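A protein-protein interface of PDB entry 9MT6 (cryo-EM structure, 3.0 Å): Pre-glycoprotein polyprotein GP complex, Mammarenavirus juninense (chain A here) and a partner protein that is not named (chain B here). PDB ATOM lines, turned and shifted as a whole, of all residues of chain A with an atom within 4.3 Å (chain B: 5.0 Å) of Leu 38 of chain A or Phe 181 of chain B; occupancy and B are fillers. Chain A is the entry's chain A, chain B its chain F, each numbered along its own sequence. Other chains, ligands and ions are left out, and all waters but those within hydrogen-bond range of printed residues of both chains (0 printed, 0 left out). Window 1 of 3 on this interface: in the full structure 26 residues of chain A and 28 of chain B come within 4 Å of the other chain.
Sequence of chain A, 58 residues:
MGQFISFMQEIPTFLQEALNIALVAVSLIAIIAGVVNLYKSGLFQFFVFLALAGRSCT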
ATOM      1  N   ILE A  31     -15.438 -16.903 -16.785  1.00  0.00           N
ATOM      2  CA  ILE A  31     -16.742 -17.056 -16.141  1.00  0.00           C
ATOM      3  C   ILE A  31     -17.015 -15.889 -15.200  1.00  0.00           C
ATOM      4  O   ILE A  31     -18.121 -15.329 -15.184  1.00  0.00           O
ATOM      5  CB  ILE A  31     -16.822 -18.407 -15.406  1.00  0.00           C
ATOM      6  CG1 ILE A  31     -16.914 -19.555 -16.408  1.00  0.00           C
ATOM      7  CG2 ILE A  31     -18.011 -18.433 -14.465  1.00  0.00           C
ATOM      8  CD1 ILE A  31     -16.659 -20.912 -15.800  1.00  0.00           C
ATOM      9  N   GLY A  34     -17.718 -12.773 -17.236  1.00  0.00           N
ATOM     10  CA  GLY A  34     -19.041 -12.872 -17.824  1.00  0.00           C
ATOM     11  C   GLY A  34     -20.135 -12.578 -16.820  1.00  0.00           C
ATOM     12  O   GLY A  34     -21.097 -11.872 -17.125  1.00  0.00           O
ATOM     13  N   VAL A  35     -19.990 -13.093 -15.598  1.00  0.00           N
ATOM     14  CA  VAL A  35     -20.980 -12.807 -14.564  1.00  0.00           C
ATOM     15  C   VAL A  35     -21.011 -11.316 -14.251  1.00  0.00           C
ATOM     16  O   VAL A  35     -22.084 -10.705 -14.157  1.00  0.00           O
ATOM     17  CB  VAL A  35     -20.703 -13.648 -13.307  1.00  0.00           C
ATOM     18  CG1 VAL A  35     -21.483 -13.106 -12.123  1.00  0.00           C
ATOM     19  CG2 VAL A  35     -21.065 -15.101 -13.560  1.00  0.00           C
ATOM     20  N   VAL A  36     -19.835 -10.698 -14.106  1.00  0.00           N
ATOM     21  CA  VAL A  36     -19.813  -9.299 -13.682  1.00  0.00           C
ATOM     22  C   VAL A  36     -20.364  -8.388 -14.774  1.00  0.00           C
ATOM     23  O   VAL A  36     -21.083  -7.426 -14.483  1.00  0.00           O
ATOM     24  CB  VAL A  36     -18.407  -8.861 -13.225  1.00  0.00           C
ATOM     25  CG1 VAL A  36     -17.887  -9.780 -12.127  1.00  0.00           C
ATOM     26  CG2 VAL A  36     -17.433  -8.771 -14.377  1.00  0.00           C
ATOM     27  N   ASN A  37     -20.075  -8.673 -16.046  1.00  0.00           N
ATOM     28  CA  ASN A  37     -20.606  -7.774 -17.063  1.00  0.00           C
ATOM     29  C   ASN A  37     -22.021  -8.141 -17.501  1.00  0.00           C
ATOM     30  O   ASN A  37     -22.689  -7.305 -18.117  1.00  0.00           O
ATOM     31  CB  ASN A  37     -19.661  -7.674 -18.267  1.00  0.00           C
ATOM     32  CG  ASN A  37     -19.371  -9.000 -18.897  1.00  0.00           C
ATOM     33  OD1 ASN A  37     -20.025  -9.989 -18.605  1.00  0.00           O
ATOM     34  ND2 ASN A  37     -18.373  -9.033 -19.771  1.00  0.00           N
ATOM     35  N   LEU A  38     -22.519  -9.337 -17.168  1.00  0.00           N
ATOM     36  CA  LEU A  38     -23.963  -9.547 -17.236  1.00  0.00           C
ATOM     37  C   LEU A  38     -24.676  -8.764 -16.143  1.00  0.00           C
ATOM     38  O   LEU A  38     -25.761  -8.217 -16.373  1.00  0.00           O
ATOM     39  CB  LEU A  38     -24.314 -11.032 -17.136  1.00  0.00           C
ATOM     40  CG  LEU A  38     -24.020 -11.936 -18.329  1.00  0.00           C
ATOM     41  CD1 LEU A  38     -24.346 -13.374 -17.986  1.00  0.00           C
ATOM     42  CD2 LEU A  38     -24.810 -11.482 -19.540  1.00  0.00           C
ATOM     43  N   TYR A  39     -24.086  -8.704 -14.947  1.00  0.00           N
ATOM     44  CA  TYR A  39     -24.647  -7.860 -13.897  1.00  0.00           C
ATOM     45  C   TYR A  39     -24.632  -6.392 -14.307  1.00  0.00           C
ATOM     46  O   TYR A  39     -25.601  -5.663 -14.070  1.00  0.00           O
ATOM     47  CB  TYR A  39     -23.882  -8.054 -12.591  1.00  0.00           C
ATOM     48  CG  TYR A  39     -24.344  -7.135 -11.484  1.00  0.00           C
ATOM     49  CD1 TYR A  39     -25.519  -7.389 -10.791  1.00  0.00           C
ATOM     50  CD2 TYR A  39     -23.608  -6.010 -11.134  1.00  0.00           C
ATOM     51  CE1 TYR A  39     -25.947  -6.551  -9.779  1.00  0.00           C
ATOM     52  CE2 TYR A  39     -24.029  -5.166 -10.125  1.00  0.00           C
ATOM     53  CZ  TYR A  39     -25.199  -5.441  -9.450  1.00  0.00           C
ATOM     54  OH  TYR A  39     -25.625  -4.607  -8.444  1.00  0.00           O
ATOM     55  N   LYS A  40     -23.535  -5.940 -14.917  1.00  0.00           N
ATOM     56  CA  LYS A  40     -23.470  -4.561 -15.389  1.00  0.00           C
ATOM     57  C   LYS A  40     -24.453  -4.314 -16.526  1.00  0.00           C
ATOM     58  O   LYS A  40     -25.014  -3.217 -16.638  1.00  0.00           O
ATOM     59  CB  LYS A  40     -22.051  -4.212 -15.828  1.00  0.00           C
ATOM     60  CG  LYS A  40     -21.058  -4.104 -14.694  1.00  0.00           C
ATOM     61  CD  LYS A  40     -19.691  -3.692 -15.205  1.00  0.00           C
ATOM     62  CE  LYS A  40     -18.687  -3.595 -14.070  1.00  0.00           C
ATOM     63  NZ  LYS A  40     -17.339  -3.199 -14.559  1.00  0.00           N
ATOM     64  N   SER A  41     -24.667  -5.311 -17.389  1.00  0.00           N
ATOM     65  CA  SER A  41     -25.591  -5.133 -18.504  1.00  0.00           C
ATOM     66  C   SER A  41     -27.011  -4.890 -18.012  1.00  0.00           C
ATOM     67  O   SER A  41     -27.717  -4.023 -18.538  1.00  0.00           O
ATOM     68  CB  SER A  41     -25.546  -6.351 -19.424  1.00  0.00           C
ATOM     69  OG  SER A  41     -26.057  -7.500 -18.777  1.00  0.00           O
ATOM     70  N   GLY A  42     -27.446  -5.642 -17.007  1.00  0.00           N
ATOM     71  CA  GLY A  42     -28.776  -5.467 -16.462  1.00  0.00           C
ATOM     72  C   GLY A  42     -29.674  -6.671 -16.646  1.00  0.00           C
ATOM     73  O   GLY A  42     -30.878  -6.596 -16.387  1.00  0.00           O
ATOM     74  N   LEU A  43     -29.102  -7.787 -17.104  1.00  0.00           N
ATOM     75  CA  LEU A  43     -29.891  -9.001 -17.281  1.00  0.00           C
ATOM     76  C   LEU A  43     -30.452  -9.492 -15.953  1.00  0.00           C
ATOM     77  O   LEU A  43     -31.626  -9.873 -15.868  1.00  0.00           O
ATOM     78  CB  LEU A  43     -29.041 -10.088 -17.935  1.00  0.00           C
ATOM     79  CG  LEU A  43     -29.804 -11.193 -18.665  1.00  0.00           C
ATOM     80  CD1 LEU A  43     -30.369 -10.675 -19.973  1.00  0.00           C
ATOM     81  CD2 LEU A  43     -28.908 -12.398 -18.901  1.00  0.00           C
ATOM     82  N   PHE A  44     -29.625  -9.497 -14.905  1.00  0.00           N
ATOM     83  CA  PHE A  44     -30.107  -9.895 -13.588  1.00  0.00           C
ATOM     84  C   PHE A  44     -31.171  -8.931 -13.084  1.00  0.00           C
ATOM     85  O   PHE A  44     -32.193  -9.356 -12.530  1.00  0.00           O
ATOM     86  CB  PHE A  44     -28.941  -9.969 -12.603  1.00  0.00           C
ATOM     87  CG  PHE A  44     -27.948 -11.048 -12.922  1.00  0.00           C
ATOM     88  CD1 PHE A  44     -28.372 -12.321 -13.257  1.00  0.00           C
ATOM     89  CD2 PHE A  44     -26.588 -10.791 -12.879  1.00  0.00           C
ATOM     90  CE1 PHE A  44     -27.461 -13.316 -13.550  1.00  0.00           C
ATOM     91  CE2 PHE A  44     -25.671 -11.783 -13.168  1.00  0.00           C
ATOM     92  CZ  PHE A  44     -26.108 -13.047 -13.504  1.00  0.00           C
ATOM     93  N   TRP B 177     -16.002 -22.762 -24.273  1.00  0.00           N
ATOM     94  CA  TRP B 177     -17.346 -22.309 -23.937  1.00  0.00           C
ATOM     95  C   TRP B 177     -17.317 -21.139 -22.965  1.00  0.00           C
ATOM     96  O   TRP B 177     -18.174 -20.253 -23.044  1.00  0.00           O
ATOM     97  CB  TRP B 177     -18.165 -23.470 -23.380  1.00  0.00           C
ATOM     98  CG  TRP B 177     -18.560 -24.440 -24.447  1.00  0.00           C
ATOM     99  CD1 TRP B 177     -18.172 -25.738 -24.559  1.00  0.00           C
ATOM    100  CD2 TRP B 177     -19.416 -24.181 -25.565  1.00  0.00           C
ATOM    101  NE1 TRP B 177     -18.731 -26.306 -25.675  1.00  0.00           N
ATOM    102  CE2 TRP B 177     -19.501 -25.370 -26.309  1.00  0.00           C
ATOM    103  CE3 TRP B 177     -20.120 -23.058 -26.008  1.00  0.00           C
ATOM    104  CZ2 TRP B 177     -20.262 -25.469 -27.469  1.00  0.00           C
ATOM    105  CZ3 TRP B 177     -20.874 -23.160 -27.157  1.00  0.00           C
ATOM    106  CH2 TRP B 177     -20.939 -24.355 -27.874  1.00  0.00           C
ATOM    107  N   SER B 178     -16.334 -21.098 -22.064  1.00  0.00           N
ATOM    108  CA  SER B 178     -16.175 -19.935 -21.202  1.00  0.00           C
ATOM    109  C   SER B 178     -15.847 -18.690 -22.014  1.00  0.00           C
ATOM    110  O   SER B 178     -16.384 -17.609 -21.750  1.00  0.00           O
ATOM    111  CB  SER B 178     -15.091 -20.203 -20.161  1.00  0.00           C
ATOM    112  OG  SER B 178     -15.427 -21.320 -19.357  1.00  0.00           O
ATOM    113  N   THR B 179     -14.974 -18.824 -23.015  1.00  0.00           N
ATOM    114  CA  THR B 179     -14.651 -17.682 -23.865  1.00  0.00           C
ATOM    115  C   THR B 179     -15.865 -17.222 -24.668  1.00  0.00           C
ATOM    116  O   THR B 179     -16.101 -16.016 -24.812  1.00  0.00           O
ATOM    117  CB  THR B 179     -13.492 -18.030 -24.794  1.00  0.00           C
ATOM    118  OG1 THR B 179     -13.772 -19.261 -25.471  1.00  0.00           O
ATOM    119  CG2 THR B 179     -12.205 -18.175 -23.998  1.00  0.00           C
ATOM    120  N   VAL B 180     -16.643 -18.167 -25.201  1.00  0.00           N
ATOM    121  CA  VAL B 180     -17.847 -17.803 -25.950  1.00  0.00           C
ATOM    122  C   VAL B 180     -18.847 -17.093 -25.046  1.00  0.00           C
ATOM    123  O   VAL B 180     -19.452 -16.080 -25.429  1.00  0.00           O
ATOM    124  CB  VAL B 180     -18.465 -19.048 -26.611  1.00  0.00           C
ATOM    125  CG1 VAL B 180     -19.792 -18.705 -27.259  1.00  0.00           C
ATOM    126  CG2 VAL B 180     -17.512 -19.628 -27.638  1.00  0.00           C
ATOM    127  N   PHE B 181     -19.037 -17.614 -23.832  1.00  0.00           N
ATOM    128  CA  PHE B 181     -19.940 -16.989 -22.875  1.00  0.00           C
ATOM    129  C   PHE B 181     -19.472 -15.587 -22.513  1.00  0.00           C
ATOM    130  O   PHE B 181     -20.282 -14.660 -22.420  1.00  0.00           O
ATOM    131  CB  PHE B 181     -20.049 -17.874 -21.636  1.00  0.00           C
ATOM    132  CG  PHE B 181     -20.584 -17.174 -20.425  1.00  0.00           C
ATOM    133  CD1 PHE B 181     -21.903 -16.774 -20.365  1.00  0.00           C
ATOM    134  CD2 PHE B 181     -19.775 -16.953 -19.330  1.00  0.00           C
ATOM    135  CE1 PHE B 181     -22.395 -16.146 -19.247  1.00  0.00           C
ATOM    136  CE2 PHE B 181     -20.264 -16.325 -18.208  1.00  0.00           C
ATOM    137  CZ  PHE B 181     -21.573 -15.923 -18.167  1.00  0.00           C
ATOM    138  N   PHE B 182     -18.164 -15.408 -22.326  1.00  0.00           N
ATOM    139  CA  PHE B 182     -17.633 -14.090 -22.003  1.00  0.00           C
ATOM    140  C   PHE B 182     -17.829 -13.107 -23.151  1.00  0.00           C
ATOM    141  O   PHE B 182     -18.134 -11.930 -22.927  1.00  0.00           O
ATOM    142  CB  PHE B 182     -16.156 -14.205 -21.640  1.00  0.00           C
ATOM    143  CG  PHE B 182     -15.489 -12.890 -21.405  1.00  0.00           C
ATOM    144  CD1 PHE B 182     -16.063 -11.949 -20.574  1.00  0.00           C
ATOM    145  CD2 PHE B 182     -14.278 -12.601 -21.995  1.00  0.00           C
ATOM    146  CE1 PHE B 182     -15.449 -10.742 -20.354  1.00  0.00           C
ATOM    147  CE2 PHE B 182     -13.659 -11.398 -21.769  1.00  0.00           C
ATOM    148  CZ  PHE B 182     -14.244 -10.471 -20.951  1.00  0.00           C
ATOM    149  N   THR B 183     -17.641 -13.564 -24.389  1.00  0.00           N
ATOM    150  CA  THR B 183     -17.828 -12.668 -25.526  1.00  0.00           C
ATOM    151  C   THR B 183     -19.291 -12.259 -25.670  1.00  0.00           C
ATOM    152  O   THR B 183     -19.600 -11.080 -25.903  1.00  0.00           O
ATOM    153  CB  THR B 183     -17.315 -13.333 -26.801  1.00  0.00           C
ATOM    154  OG1 THR B 183     -15.945 -13.707 -26.621  1.00  0.00           O
ATOM    155  CG2 THR B 183     -17.393 -12.368 -27.958  1.00  0.00           C
ATOM    156  N   ALA B 184     -20.209 -13.215 -25.514  1.00  0.00           N
ATOM    157  CA  ALA B 184     -21.629 -12.876 -25.524  1.00  0.00           C
ATOM    158  C   ALA B 184     -21.972 -11.931 -24.381  1.00  0.00           C
ATOM    159  O   ALA B 184     -22.829 -11.048 -24.524  1.00  0.00           O
ATOM    160  CB  ALA B 184     -22.472 -14.148 -25.442  1.00  0.00           C
ATOM    161  N   SER B 185     -21.309 -12.100 -23.239  1.00  0.00           N
ATOM    162  CA  SER B 185     -21.532 -11.216 -22.103  1.00  0.00           C
ATOM    163  C   SER B 185     -21.064  -9.796 -22.400  1.00  0.00           C
ATOM    164  O   SER B 185     -21.727  -8.828 -22.014  1.00  0.00           O
ATOM    165  CB  SER B 185     -20.828 -11.781 -20.876  1.00  0.00           C
ATOM    166  OG  SER B 185     -19.479 -11.352 -20.823  1.00  0.00           O
ATOM    167  N   LEU B 188     -23.757  -8.267 -24.544  1.00  0.00           N
ATOM    168  CA  LEU B 188     -24.898  -7.829 -23.747  1.00  0.00           C
ATOM    169  C   LEU B 188     -24.553  -6.595 -22.925  1.00  0.00           C
ATOM    170  O   LEU B 188     -25.417  -5.752 -22.660  1.00  0.00           O
ATOM    171  CB  LEU B 188     -25.375  -8.961 -22.842  1.00  0.00           C
ATOM    172  CG  LEU B 188     -26.063 -10.123 -23.552  1.00  0.00           C
ATOM    173  CD1 LEU B 188     -26.797 -11.003 -22.561  1.00  0.00           C
ATOM    174  CD2 LEU B 188     -27.010  -9.610 -24.623  1.00  0.00           C
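The backbone carbonyl oxygen (O) of Gly 34 of chain A lies close to the side-chain amide oxygen (OD1) of Asn 37 of chain A, at 2.6 Å. The backbone carbonyl oxygen (O) of Asn 37 of chain A lies close to the side-chain hydroxyl (OG) of Ser 41 of chain A (3.4 Å). O of Leu 38 of chain A is in hydrogen-bond range of OG of Ser 41 of chain A (2.5 Å). O of Leu 38 of chain A is in hydrogen-bond range of N of Leu 43 of chain A, at 3.4 Å. OG of Ser 41 of chain A sits at hydrogen-bond distance from N of Leu 43 of chain A (3.5 Å). The backbone carbonyl oxygen (O) of Phe 182 of chain B lies within hydrogen-bond range of the side-chain hydroxyl (OG) of Ser 185 of chain B, at 2.6 Å.
Of chain B, only Phe 181 (3.6 Å) and Leu 188 (3.6 Å) come within 4 Å of Leu 38 of chain A. Of the printed residues of chain A, Phe 181 of chain B touches Ile 31, Gly 34 and Leu 38. Of the printed residues of chain B, Asn 37 of chain A touches Phe 182 (3.4 Å) and Ser 185 (2.7 Å). Printed residues of chain B within 4 Å of Ile 31 of chain A: Ser 178 (3.7 Å) and Phe 181 (3.8 Å). Of the printed residues of chain B, Gly 34 of chain A touches Phe 181, Phe 182 and Ser 185. Of the printed residues of chain A, Ser 178 of chain B touches Ile 31. Of the printed residues of chain A, Ser 185 of chain B touches Gly 34 and Asn 37.
The side-chain amide oxygen (OD1) of Asn 37 of chain A lies within hydrogen-bond range of the side-chain hydroxyl (OG) of Ser 185 of chain B, 2.7 Å away.
Of the 12 printed residues of chain A, 5 touch a printed residue of chain B. Printed residues of chain A that touch a printed residue of chain B: Ile 31, Gly 34, Asn 37, Leu 38 and Ser 41. Hydrophobic or aromatic side chains of chain B within 4 Å of the printed part of chain A: Phe 181, Phe 182 and Leu 188. Among the printed residues, 10 pairs touch across the chains.
Among the printed residues, merely in contact across the chains: Ile 31 of chain A with Ser 178 of chain B, Ile 31 of chain A with Phe 181 of chain B, Gly 34 of chain A with Phe 181 of chain B, Gly 34 of chain A with Phe 182 of chain B, Gly 34 of chain A with Ser 185 of chain B, Asn 37 of chain A with Phe 182 of chain B, Leu 38 of chain A with Phe 181 of chain B, Leu 38 of chain A with Leu 188 of chain B and Ser 41 of chain A with Leu 188 of chain B.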
